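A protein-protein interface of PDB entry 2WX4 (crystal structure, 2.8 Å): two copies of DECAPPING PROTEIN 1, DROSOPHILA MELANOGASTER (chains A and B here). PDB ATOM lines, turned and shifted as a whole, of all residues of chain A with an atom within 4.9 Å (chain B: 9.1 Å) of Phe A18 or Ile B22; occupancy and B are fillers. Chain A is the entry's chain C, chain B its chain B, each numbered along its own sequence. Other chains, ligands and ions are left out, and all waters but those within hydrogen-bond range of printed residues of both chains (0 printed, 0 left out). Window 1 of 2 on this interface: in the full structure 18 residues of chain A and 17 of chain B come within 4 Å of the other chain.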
ATOM      1  N   PHE A  14      13.360 -12.231  20.255  1.00  0.00           N
ATOM      2  CA  PHE A  14      13.156 -12.765  21.584  1.00  0.00           C
ATOM      3  C   PHE A  14      12.573 -14.172  21.491  1.00  0.00           C
ATOM      4  O   PHE A  14      13.099 -15.094  22.114  1.00  0.00           O
ATOM      5  CB  PHE A  14      12.236 -11.843  22.390  1.00  0.00           C
ATOM      6  CG  PHE A  14      11.924 -12.353  23.753  1.00  0.00           C
ATOM      7  CD1 PHE A  14      12.917 -12.408  24.734  1.00  0.00           C
ATOM      8  CD2 PHE A  14      10.647 -12.801  24.063  1.00  0.00           C
ATOM      9  CE1 PHE A  14      12.647 -12.909  26.013  1.00  0.00           C
ATOM     10  CE2 PHE A  14      10.355 -13.292  25.351  1.00  0.00           C
ATOM     11  CZ  PHE A  14      11.362 -13.338  26.330  1.00  0.00           C
ATOM     12  N   VAL A  15      11.515 -14.347  20.699  1.00  0.00           N
ATOM     13  CA  VAL A  15      10.886 -15.651  20.591  1.00  0.00           C
ATOM     14  C   VAL A  15      11.826 -16.679  19.970  1.00  0.00           C
ATOM     15  O   VAL A  15      11.842 -17.832  20.394  1.00  0.00           O
ATOM     16  CB  VAL A  15       9.545 -15.586  19.852  1.00  0.00           C
ATOM     17  CG1 VAL A  15       9.098 -16.977  19.416  1.00  0.00           C
ATOM     18  CG2 VAL A  15       8.494 -14.940  20.749  1.00  0.00           C
ATOM     19  N   GLN A  16      12.629 -16.253  18.995  1.00  0.00           N
ATOM     20  CA  GLN A  16      13.636 -17.135  18.385  1.00  0.00           C
ATOM     21  C   GLN A  16      14.643 -17.626  19.418  1.00  0.00           C
ATOM     22  O   GLN A  16      14.874 -18.820  19.533  1.00  0.00           O
ATOM     23  CB  GLN A  16      14.374 -16.452  17.219  1.00  0.00           C
ATOM     24  CG  GLN A  16      15.488 -17.303  16.609  1.00  0.00           C
ATOM     25  CD  GLN A  16      16.234 -16.638  15.441  1.00  0.00           C
ATOM     26  OE1 GLN A  16      16.810 -15.531  15.564  1.00  0.00           O
ATOM     27  NE2 GLN A  16      16.252 -17.333  14.303  1.00  0.00           N
ATOM     28  N   ALA A  17      15.214 -16.702  20.182  1.00  0.00           N
ATOM     29  CA  ALA A  17      16.289 -17.021  21.104  1.00  0.00           C
ATOM     30  C   ALA A  17      15.805 -17.926  22.222  1.00  0.00           C
ATOM     31  O   ALA A  17      16.496 -18.857  22.626  1.00  0.00           O
ATOM     32  CB  ALA A  17      16.866 -15.765  21.669  1.00  0.00           C
ATOM     33  N   PHE A  18      14.606 -17.641  22.704  1.00  0.00           N
ATOM     34  CA  PHE A  18      13.979 -18.388  23.785  1.00  0.00           C
ATOM     35  C   PHE A  18      13.785 -19.850  23.377  1.00  0.00           C
ATOM     36  O   PHE A  18      14.246 -20.772  24.061  1.00  0.00           O
ATOM     37  CB  PHE A  18      12.621 -17.750  24.102  1.00  0.00           C
ATOM     38  CG  PHE A  18      12.206 -17.879  25.531  1.00  0.00           C
ATOM     39  CD1 PHE A  18      11.853 -19.114  26.066  1.00  0.00           C
ATOM     40  CD2 PHE A  18      12.149 -16.764  26.339  1.00  0.00           C
ATOM     41  CE1 PHE A  18      11.470 -19.225  27.394  1.00  0.00           C
ATOM     42  CE2 PHE A  18      11.761 -16.867  27.656  1.00  0.00           C
ATOM     43  CZ  PHE A  18      11.425 -18.100  28.182  1.00  0.00           C
ATOM     44  N   THR A  19      13.100 -20.034  22.248  1.00  0.00           N
ATOM     45  CA  THR A  19      12.878 -21.339  21.653  1.00  0.00           C
ATOM     46  C   THR A  19      14.186 -22.103  21.541  1.00  0.00           C
ATOM     47  O   THR A  19      14.267 -23.250  21.944  1.00  0.00           O
ATOM     48  CB  THR A  19      12.223 -21.208  20.265  1.00  0.00           C
ATOM     49  OG1 THR A  19      10.970 -20.544  20.409  1.00  0.00           O
ATOM     50  CG2 THR A  19      11.938 -22.577  19.672  1.00  0.00           C
ATOM     51  N   TYR A  20      15.217 -21.465  21.008  1.00  0.00           N
ATOM     52  CA  TYR A  20      16.487 -22.132  20.902  1.00  0.00           C
ATOM     53  C   TYR A  20      16.968 -22.592  22.274  1.00  0.00           C
ATOM     54  O   TYR A  20      17.300 -23.759  22.468  1.00  0.00           O
ATOM     55  CB  TYR A  20      17.531 -21.242  20.242  1.00  0.00           C
ATOM     56  CG  TYR A  20      18.845 -21.973  20.094  1.00  0.00           C
ATOM     57  CD1 TYR A  20      19.027 -22.899  19.063  1.00  0.00           C
ATOM     58  CD2 TYR A  20      19.885 -21.776  21.003  1.00  0.00           C
ATOM     59  CE1 TYR A  20      20.209 -23.599  18.927  1.00  0.00           C
ATOM     60  CE2 TYR A  20      21.084 -22.468  20.871  1.00  0.00           C
ATOM     61  CZ  TYR A  20      21.235 -23.386  19.826  1.00  0.00           C
ATOM     62  OH  TYR A  20      22.414 -24.096  19.682  1.00  0.00           O
ATOM     63  N   LEU A  21      16.973 -21.666  23.229  1.00  0.00           N
ATOM     64  CA  LEU A  21      17.480 -21.941  24.574  1.00  0.00           C
ATOM     65  C   LEU A  21      16.704 -23.010  25.327  1.00  0.00           C
ATOM     66  O   LEU A  21      17.300 -23.837  26.020  1.00  0.00           O
ATOM     67  CB  LEU A  21      17.576 -20.660  25.399  1.00  0.00           C
ATOM     68  CG  LEU A  21      18.739 -19.779  24.939  1.00  0.00           C
ATOM     69  CD1 LEU A  21      18.786 -18.514  25.754  1.00  0.00           C
ATOM     70  CD2 LEU A  21      20.062 -20.522  25.028  1.00  0.00           C
ATOM     71  N   ILE A  22      15.384 -23.012  25.178  1.00  0.00           N
ATOM     72  CA  ILE A  22      14.577 -23.987  25.890  1.00  0.00           C
ATOM     73  C   ILE A  22      14.729 -25.375  25.254  1.00  0.00           C
ATOM     74  O   ILE A  22      14.401 -26.398  25.864  1.00  0.00           O
ATOM     75  CB  ILE A  22      13.099 -23.541  26.020  1.00  0.00           C
ATOM     76  CG1 ILE A  22      12.335 -24.502  26.931  1.00  0.00           C
ATOM     77  CG2 ILE A  22      12.436 -23.416  24.653  1.00  0.00           C
ATOM     78  CD1 ILE A  22      11.062 -23.962  27.451  1.00  0.00           C
ATOM     79  N   GLN A  23      15.265 -25.407  24.039  1.00  0.00           N
ATOM     80  CA  GLN A  23      15.356 -26.648  23.290  1.00  0.00           C
ATOM     81  C   GLN A  23      16.729 -27.267  23.360  1.00  0.00           C
ATOM     82  O   GLN A  23      16.882 -28.425  23.045  1.00  0.00           O
ATOM     83  CB  GLN A  23      14.941 -26.436  21.837  1.00  0.00           C
ATOM     84  CG  GLN A  23      13.516 -26.849  21.565  1.00  0.00           C
ATOM     85  CD  GLN A  23      12.922 -26.196  20.331  1.00  0.00           C
ATOM     86  OE1 GLN A  23      11.701 -26.088  20.212  1.00  0.00           O
ATOM     87  NE2 GLN A  23      13.772 -25.749  19.413  1.00  0.00           N
ATOM     88  N   PHE A  28      18.140 -24.620  31.661  1.00  0.00           N
ATOM     89  CA  PHE A  28      17.164 -23.578  31.390  1.00  0.00           C
ATOM     90  C   PHE A  28      15.759 -24.131  31.354  1.00  0.00           C
ATOM     91  O   PHE A  28      14.849 -23.568  31.956  1.00  0.00           O
ATOM     92  CB  PHE A  28      17.497 -22.908  30.055  1.00  0.00           C
ATOM     93  CG  PHE A  28      16.682 -21.683  29.763  1.00  0.00           C
ATOM     94  CD1 PHE A  28      16.770 -20.563  30.572  1.00  0.00           C
ATOM     95  CD2 PHE A  28      15.827 -21.653  28.670  1.00  0.00           C
ATOM     96  CE1 PHE A  28      16.030 -19.440  30.300  1.00  0.00           C
ATOM     97  CE2 PHE A  28      15.069 -20.522  28.391  1.00  0.00           C
ATOM     98  CZ  PHE A  28      15.169 -19.418  29.208  1.00  0.00           C
ATOM     99  N   LEU A  32      12.413 -23.712  34.089  1.00  0.00           N
ATOM    100  CA  LEU A  32      11.092 -23.280  33.637  1.00  0.00           C
ATOM    101  C   LEU A  32      10.036 -24.334  33.933  1.00  0.00           C
ATOM    102  O   LEU A  32       8.904 -24.003  34.298  1.00  0.00           O
ATOM    103  CB  LEU A  32      11.103 -22.969  32.142  1.00  0.00           C
ATOM    104  CG  LEU A  32      11.925 -21.784  31.645  1.00  0.00           C
ATOM    105  CD1 LEU A  32      11.821 -21.754  30.163  1.00  0.00           C
ATOM    106  CD2 LEU A  32      11.404 -20.511  32.218  1.00  0.00           C
ATOM    107  N   PHE B  14       6.479 -30.566  28.303  1.00  0.00           N
ATOM    108  CA  PHE B  14       6.493 -29.139  28.630  1.00  0.00           C
ATOM    109  C   PHE B  14       7.264 -28.333  27.582  1.00  0.00           C
ATOM    110  O   PHE B  14       6.781 -27.295  27.140  1.00  0.00           O
ATOM    111  CB  PHE B  14       7.063 -28.934  30.053  1.00  0.00           C
ATOM    112  CG  PHE B  14       7.374 -27.497  30.409  1.00  0.00           C
ATOM    113  CD1 PHE B  14       6.372 -26.649  30.896  1.00  0.00           C
ATOM    114  CD2 PHE B  14       8.675 -27.005  30.286  1.00  0.00           C
ATOM    115  CE1 PHE B  14       6.659 -25.319  31.228  1.00  0.00           C
ATOM    116  CE2 PHE B  14       8.967 -25.695  30.608  1.00  0.00           C
ATOM    117  CZ  PHE B  14       7.960 -24.845  31.084  1.00  0.00           C
ATOM    118  N   VAL B  15       8.444 -28.805  27.175  1.00  0.00           N
ATOM    119  CA  VAL B  15       9.230 -28.076  26.178  1.00  0.00           C
ATOM    120  C   VAL B  15       8.422 -27.906  24.905  1.00  0.00           C
ATOM    121  O   VAL B  15       8.309 -26.801  24.392  1.00  0.00           O
ATOM    122  CB  VAL B  15      10.594 -28.718  25.896  1.00  0.00           C
ATOM    123  CG1 VAL B  15      11.206 -28.148  24.648  1.00  0.00           C
ATOM    124  CG2 VAL B  15      11.514 -28.477  27.056  1.00  0.00           C
ATOM    125  N   GLN B  16       7.823 -28.998  24.433  1.00  0.00           N
ATOM    126  CA  GLN B  16       6.983 -28.989  23.242  1.00  0.00           C
ATOM    127  C   GLN B  16       5.834 -28.017  23.384  1.00  0.00           C
ATOM    128  O   GLN B  16       5.575 -27.228  22.478  1.00  0.00           O
ATOM    129  CB  GLN B  16       6.401 -30.366  22.984  1.00  0.00           C
ATOM    130  CG  GLN B  16       7.360 -31.405  22.420  1.00  0.00           C
ATOM    131  CD  GLN B  16       6.700 -32.792  22.360  1.00  0.00           C
ATOM    132  OE1 GLN B  16       5.461 -32.925  22.464  1.00  0.00           O
ATOM    133  NE2 GLN B  16       7.518 -33.834  22.218  1.00  0.00           N
ATOM    134  N   ALA B  17       5.138 -28.083  24.512  1.00  0.00           N
ATOM    135  CA  ALA B  17       4.008 -27.196  24.754  1.00  0.00           C
ATOM    136  C   ALA B  17       4.462 -25.742  24.825  1.00  0.00           C
ATOM    137  O   ALA B  17       3.825 -24.866  24.226  1.00  0.00           O
ATOM    138  CB  ALA B  17       3.263 -27.590  26.011  1.00  0.00           C
ATOM    139  N   PHE B  18       5.568 -25.492  25.529  1.00  0.00           N
ATOM    140  CA  PHE B  18       6.044 -24.129  25.747  1.00  0.00           C
ATOM    141  C   PHE B  18       6.477 -23.554  24.406  1.00  0.00           C
ATOM    142  O   PHE B  18       6.043 -22.452  24.034  1.00  0.00           O
ATOM    143  CB  PHE B  18       7.190 -24.080  26.774  1.00  0.00           C
ATOM    144  CG  PHE B  18       7.354 -22.743  27.428  1.00  0.00           C
ATOM    145  CD1 PHE B  18       8.114 -21.748  26.831  1.00  0.00           C
ATOM    146  CD2 PHE B  18       6.730 -22.465  28.638  1.00  0.00           C
ATOM    147  CE1 PHE B  18       8.252 -20.491  27.441  1.00  0.00           C
ATOM    148  CE2 PHE B  18       6.862 -21.209  29.260  1.00  0.00           C
ATOM    149  CZ  PHE B  18       7.616 -20.226  28.662  1.00  0.00           C
ATOM    150  N   THR B  19       7.301 -24.316  23.677  1.00  0.00           N
ATOM    151  CA  THR B  19       7.731 -23.936  22.338  1.00  0.00           C
ATOM    152  C   THR B  19       6.539 -23.562  21.488  1.00  0.00           C
ATOM    153  O   THR B  19       6.562 -22.541  20.799  1.00  0.00           O
ATOM    154  CB  THR B  19       8.436 -25.069  21.613  1.00  0.00           C
ATOM    155  OG1 THR B  19       9.694 -25.328  22.238  1.00  0.00           O
ATOM    156  CG2 THR B  19       8.665 -24.698  20.162  1.00  0.00           C
ATOM    157  N   TYR B  20       5.499 -24.392  21.528  1.00  0.00           N
ATOM    158  CA  TYR B  20       4.321 -24.101  20.743  1.00  0.00           C
ATOM    159  C   TYR B  20       3.662 -22.829  21.243  1.00  0.00           C
ATOM    160  O   TYR B  20       3.419 -21.927  20.453  1.00  0.00           O
ATOM    161  CB  TYR B  20       3.346 -25.279  20.681  1.00  0.00           C
ATOM    162  CG  TYR B  20       2.141 -24.992  19.808  1.00  0.00           C
ATOM    163  CD1 TYR B  20       2.183 -25.192  18.422  1.00  0.00           C
ATOM    164  CD2 TYR B  20       0.958 -24.502  20.372  1.00  0.00           C
ATOM    165  CE1 TYR B  20       1.068 -24.913  17.619  1.00  0.00           C
ATOM    166  CE2 TYR B  20      -0.163 -24.218  19.588  1.00  0.00           C
ATOM    167  CZ  TYR B  20      -0.105 -24.426  18.214  1.00  0.00           C
ATOM    168  OH  TYR B  20      -1.228 -24.142  17.458  1.00  0.00           O
ATOM    169  N   LEU B  21       3.425 -22.733  22.549  1.00  0.00           N
ATOM    170  CA  LEU B  21       2.775 -21.554  23.135  1.00  0.00           C
ATOM    171  C   LEU B  21       3.424 -20.238  22.683  1.00  0.00           C
ATOM    172  O   LEU B  21       2.765 -19.368  22.102  1.00  0.00           O
ATOM    173  CB  LEU B  21       2.770 -21.647  24.664  1.00  0.00           C
ATOM    174  CG  LEU B  21       1.718 -20.818  25.409  1.00  0.00           C
ATOM    175  CD1 LEU B  21       0.321 -21.302  25.020  1.00  0.00           C
ATOM    176  CD2 LEU B  21       1.913 -20.824  26.953  1.00  0.00           C
ATOM    177  N   ILE B  22       4.727 -20.122  22.923  1.00  0.00           N
ATOM    178  CA  ILE B  22       5.452 -18.877  22.727  1.00  0.00           C
ATOM    179  C   ILE B  22       5.468 -18.489  21.259  1.00  0.00           C
ATOM    180  O   ILE B  22       5.642 -17.318  20.914  1.00  0.00           O
ATOM    181  CB  ILE B  22       6.893 -18.974  23.300  1.00  0.00           C
ATOM    182  CG1 ILE B  22       7.443 -17.583  23.627  1.00  0.00           C
ATOM    183  CG2 ILE B  22       7.836 -19.786  22.385  1.00  0.00           C
ATOM    184  CD1 ILE B  22       8.817 -17.604  24.277  1.00  0.00           C
ATOM    185  N   GLN B  23       5.261 -19.476  20.395  1.00  0.00           N
ATOM    186  CA  GLN B  23       5.278 -19.229  18.962  1.00  0.00           C
ATOM    187  C   GLN B  23       3.925 -18.864  18.376  1.00  0.00           C
ATOM    188  O   GLN B  23       3.859 -18.376  17.257  1.00  0.00           O
ATOM    189  CB  GLN B  23       5.858 -20.420  18.223  1.00  0.00           C
ATOM    190  CG  GLN B  23       7.363 -20.483  18.306  1.00  0.00           C
ATOM    191  CD  GLN B  23       7.911 -21.750  17.727  1.00  0.00           C
ATOM    192  OE1 GLN B  23       7.165 -22.683  17.396  1.00  0.00           O
ATOM    193  NE2 GLN B  23       9.231 -21.806  17.595  1.00  0.00           N
ATOM    194  N   ASN B  24       2.857 -19.066  19.138  1.00  0.00           N
ATOM    195  CA  ASN B  24       1.523 -18.936  18.594  1.00  0.00           C
ATOM    196  C   ASN B  24       0.627 -17.996  19.369  1.00  0.00           C
ATOM    197  O   ASN B  24      -0.138 -17.234  18.786  1.00  0.00           O
ATOM    198  CB  ASN B  24       0.876 -20.312  18.503  1.00  0.00           C
ATOM    199  CG  ASN B  24       1.306 -21.070  17.267  1.00  0.00           C
ATOM    200  OD1 ASN B  24       0.617 -21.028  16.247  1.00  0.00           O
ATOM    201  ND2 ASN B  24       2.454 -21.754  17.337  1.00  0.00           N
ATOM    202  N   ASP B  25       0.697 -18.070  20.690  1.00  0.00           N
ATOM    203  CA  ASP B  25      -0.042 -17.151  21.535  1.00  0.00           C
ATOM    204  C   ASP B  25       0.783 -15.868  21.667  1.00  0.00           C
ATOM    205  O   ASP B  25       1.820 -15.847  22.340  1.00  0.00           O
ATOM    206  CB  ASP B  25      -0.314 -17.800  22.889  1.00  0.00           C
ATOM    207  CG  ASP B  25      -1.101 -16.910  23.809  1.00  0.00           C
ATOM    208  OD1 ASP B  25      -0.741 -15.727  23.960  1.00  0.00           O
ATOM    209  OD2 ASP B  25      -2.080 -17.393  24.397  1.00  0.00           O
ATOM    210  N   LYS B  26       0.335 -14.809  20.999  1.00  0.00           N
ATOM    211  CA  LYS B  26       1.074 -13.543  21.016  1.00  0.00           C
ATOM    212  C   LYS B  26       0.953 -12.815  22.346  1.00  0.00           C
ATOM    213  O   LYS B  26       1.900 -12.170  22.792  1.00  0.00           O
ATOM    214  CB  LYS B  26       0.659 -12.620  19.863  1.00  0.00           C
ATOM    215  CG  LYS B  26       1.720 -12.539  18.761  1.00  0.00           C
ATOM    216  CD  LYS B  26       1.526 -11.322  17.835  1.00  0.00           C
ATOM    217  CE  LYS B  26       2.485 -11.392  16.635  1.00  0.00           C
ATOM    218  NZ  LYS B  26       1.971 -10.622  15.466  1.00  0.00           N
ATOM    219  N   GLU B  27      -0.216 -12.921  22.971  1.00  0.00           N
ATOM    220  CA  GLU B  27      -0.443 -12.346  24.293  1.00  0.00           C
ATOM    221  C   GLU B  27       0.615 -12.849  25.290  1.00  0.00           C
ATOM    222  O   GLU B  27       1.266 -12.043  25.972  1.00  0.00           O
ATOM    223  CB  GLU B  27      -1.871 -12.652  24.770  1.00  0.00           C
ATOM    224  CG  GLU B  27      -2.271 -11.985  26.084  1.00  0.00           C
ATOM    225  CD  GLU B  27      -3.789 -11.891  26.272  1.00  0.00           C
ATOM    226  OE1 GLU B  27      -4.507 -11.701  25.255  1.00  0.00           O
ATOM    227  OE2 GLU B  27      -4.257 -11.995  27.439  1.00  0.00           O
ATOM    228  N   PHE B  28       0.806 -14.167  25.339  1.00  0.00           N
ATOM    229  CA  PHE B  28       1.786 -14.775  26.242  1.00  0.00           C
ATOM    230  C   PHE B  28       3.253 -14.457  25.913  1.00  0.00           C
ATOM    231  O   PHE B  28       4.040 -14.172  26.810  1.00  0.00           O
ATOM    232  CB  PHE B  28       1.596 -16.291  26.359  1.00  0.00           C
ATOM    233  CG  PHE B  28       2.502 -16.910  27.365  1.00  0.00           C
ATOM    234  CD1 PHE B  28       2.373 -16.575  28.731  1.00  0.00           C
ATOM    235  CD2 PHE B  28       3.520 -17.768  26.970  1.00  0.00           C
ATOM    236  CE1 PHE B  28       3.228 -17.107  29.700  1.00  0.00           C
ATOM    237  CE2 PHE B  28       4.384 -18.316  27.925  1.00  0.00           C
ATOM    238  CZ  PHE B  28       4.240 -17.973  29.298  1.00  0.00           C
ATOM    239  N   ALA B  29       3.620 -14.521  24.638  1.00  0.00           N
ATOM    240  CA  ALA B  29       4.971 -14.187  24.229  1.00  0.00           C
ATOM    241  C   ALA B  29       5.329 -12.779  24.670  1.00  0.00           C
ATOM    242  O   ALA B  29       6.443 -12.527  25.141  1.00  0.00           O
ATOM    243  CB  ALA B  29       5.120 -14.323  22.741  1.00  0.00           C
ATOM    244  N   ASN B  30       4.374 -11.860  24.535  1.00  0.00           N
ATOM    245  CA  ASN B  30       4.628 -10.455  24.845  1.00  0.00           C
ATOM    246  C   ASN B  30       4.780 -10.256  26.341  1.00  0.00           C
ATOM    247  O   ASN B  30       5.592  -9.448  26.795  1.00  0.00           O
ATOM    248  CB  ASN B  30       3.559  -9.546  24.227  1.00  0.00           C
ATOM    249  CG  ASN B  30       3.788  -9.313  22.725  1.00  0.00           C
ATOM    250  OD1 ASN B  30       4.680  -9.903  22.114  1.00  0.00           O
ATOM    251  ND2 ASN B  30       2.986  -8.443  22.131  1.00  0.00           N
ATOM    252  N   LYS B  31       4.018 -11.038  27.099  1.00  0.00           N
ATOM    253  CA  LYS B  31       4.114 -11.045  28.548  1.00  0.00           C
ATOM    254  C   LYS B  31       5.536 -11.419  28.967  1.00  0.00           C
ATOM    255  O   LYS B  31       6.170 -10.690  29.719  1.00  0.00           O
ATOM    256  CB  LYS B  31       3.094 -12.019  29.119  1.00  0.00           C
ATOM    257  CG  LYS B  31       2.626 -11.687  30.495  1.00  0.00           C
ATOM    258  CD  LYS B  31       1.204 -12.161  30.694  1.00  0.00           C
ATOM    259  CE  LYS B  31       0.896 -12.362  32.175  1.00  0.00           C
ATOM    260  NZ  LYS B  31      -0.584 -12.419  32.410  1.00  0.00           N
ATOM    261  N   LEU B  32       6.042 -12.539  28.454  1.00  0.00           N
ATOM    262  CA  LEU B  32       7.426 -12.909  28.658  1.00  0.00           C
ATOM    263  C   LEU B  32       8.380 -11.827  28.164  1.00  0.00           C
ATOM    264  O   LEU B  32       9.406 -11.558  28.793  1.00  0.00           O
ATOM    265  CB  LEU B  32       7.742 -14.218  27.946  1.00  0.00           C
ATOM    266  CG  LEU B  32       7.368 -15.507  28.676  1.00  0.00           C
ATOM    267  CD1 LEU B  32       7.544 -16.724  27.776  1.00  0.00           C
ATOM    268  CD2 LEU B  32       8.215 -15.647  29.903  1.00  0.00           C
ATOM    269  N   HIS B  33       8.054 -11.208  27.036  1.00  0.00           N
ATOM    270  CA  HIS B  33       8.937 -10.195  26.477  1.00  0.00           C
ATOM    271  C   HIS B  33       9.020  -8.966  27.377  1.00  0.00           C
ATOM    272  O   HIS B  33      10.092  -8.404  27.556  1.00  0.00           O
ATOM    273  CB  HIS B  33       8.500  -9.818  25.066  1.00  0.00           C
ATOM    274  CG  HIS B  33       9.445  -8.888  24.371  1.00  0.00           C
ATOM    275  ND1 HIS B  33       9.052  -7.667  23.873  1.00  0.00           N
ATOM    276  CD2 HIS B  33      10.770  -8.995  24.102  1.00  0.00           C
ATOM    277  CE1 HIS B  33      10.093  -7.065  23.323  1.00  0.00           C
ATOM    278  NE2 HIS B  33      11.147  -7.848  23.452  1.00  0.00           N
ATOM    279  N   ALA B  35       8.415  -9.023  30.762  1.00  0.00           N
ATOM    280  CA  ALA B  35       9.293  -9.562  31.803  1.00  0.00           C
ATOM    281  C   ALA B  35      10.751  -9.283  31.456  1.00  0.00           C
ATOM    282  O   ALA B  35      11.464  -8.656  32.233  1.00  0.00           O
ATOM    283  CB  ALA B  35       9.073 -11.055  31.998  1.00  0.00           C
ATOM    284  N   TYR B  36      11.164  -9.732  30.273  1.00  0.00           N
ATOM    285  CA  TYR B  36      12.526  -9.558  29.754  1.00  0.00           C
ATOM    286  C   TYR B  36      12.988  -8.099  29.669  1.00  0.00           C
ATOM    287  O   TYR B  36      14.078  -7.773  30.103  1.00  0.00           O
ATOM    288  CB  TYR B  36      12.642 -10.232  28.379  1.00  0.00           C
ATOM    289  CG  TYR B  36      13.837  -9.807  27.557  1.00  0.00           C
ATOM    290  CD1 TYR B  36      15.109 -10.283  27.841  1.00  0.00           C
ATOM    291  CD2 TYR B  36      13.692  -8.923  26.485  1.00  0.00           C
ATOM    292  CE1 TYR B  36      16.214  -9.875  27.076  1.00  0.00           C
ATOM    293  CE2 TYR B  36      14.802  -8.509  25.712  1.00  0.00           C
ATOM    294  CZ  TYR B  36      16.047  -8.989  26.015  1.00  0.00           C
ATOM    295  OH  TYR B  36      17.129  -8.606  25.256  1.00  0.00           O
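The side-chain amide oxygen of Gln A23 is in hydrogen-bond range of the side-chain hydroxyl of Thr B19.
The backbone carbonyl oxygen of Val B15 is in hydrogen-bond range of the side-chain hydroxyl of Thr B19, at 3.0 Å. The side-chain amide oxygen (OE1) of Gln B23 sits close to the backbone carbonyl oxygen (O) of Thr B19 (3.5 Å). The backbone carbonyl oxygen (O) of Val A15 sits at hydrogen-bond distance from the side-chain hydroxyl (OG1) of Thr A19 (2.8 Å).
CE2 of Phe A14 touches O of Ala B29, at 3.99 Å. CZ of Phe A14 touches O of Leu B32, 3.6 Å away. Phe A14 touches His B33 (CE2 to N, 3.5 Å). Tyr B36 touches Phe A14 (CB to CE1, 3.6 Å). CE1 of Phe B18 touches CE1 of Phe A18, 3.5 Å away. CD1 of Ile B22 touches CG of Phe A18, 3.6 Å away. Thr A19 touches Thr B19 (CG2 to CG2, 3.9 Å). Gln B23 touches Thr A19 (NE2 to CG2, 3.5 Å). Ile A22 touches Phe B18. O of Leu A32 touches CZ of Phe B14, at 3.5 Å.
Of chain B, only Ile B22 (3.7 Å) and Ala B29 (3.97 Å) come within 4 Å of Val A15. No residue of chain B comes within 4 Å of Ala A17. Phe A18 touches just these residues of chain B: Phe B18 and Ile B22. Of chain B, only Thr B19 (3.9 Å), Ile B22 (3.8 Å) and Gln B23 (3.5 Å) come within 4 Å of Thr A19. Of the printed residues of chain B, Leu A32 touches Phe B14. Of the printed residues of chain A, Phe B18 touches Phe A18 and Ile A22. Of the printed residues of chain A, Ile B22 touches Val A15, Phe A18 and Thr A19. Lys B26 touches none of the printed residues of chain A. Lys B31 touches none of the printed residues of chain A. Of the printed residues of chain A, Leu B32 touches Phe A14 (3.6 Å). The nearest residue of chain A that does not touch Ile B22 is Phe A14 (4.7 Å). The nearest printed residue of chain A that does not touch Phe B18 is Leu A32 (4.7 Å).
Hydrophobic or aromatic side chains of chain B that line the printed part of chain A: Phe B14, Val B15, Phe B18, Ile B22, Ala B29, Leu B32, His B33 and Tyr B36. Among the printed residues, 15 pairs touch across the chains. Among the printed residues, no Asp or Glu carboxylate lies within 4 Å of a Lys or Arg side-chain nitrogen of the other chain.
Phe A18 touches its own counterpart, Phe B18. Thr B19 touches its own counterpart, Thr A19. Thr A19 touches Ile B22, but with the chains exchanged Ile A22 does not touch Thr B19 (4.1 Å). Thr A19 touches Gln B23, and with the chains exchanged Gln A23 touches Thr B19. Of the 15 pairs that touch across the chains among the printed residues, 10 have their exchanged pair printed and touching as well.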
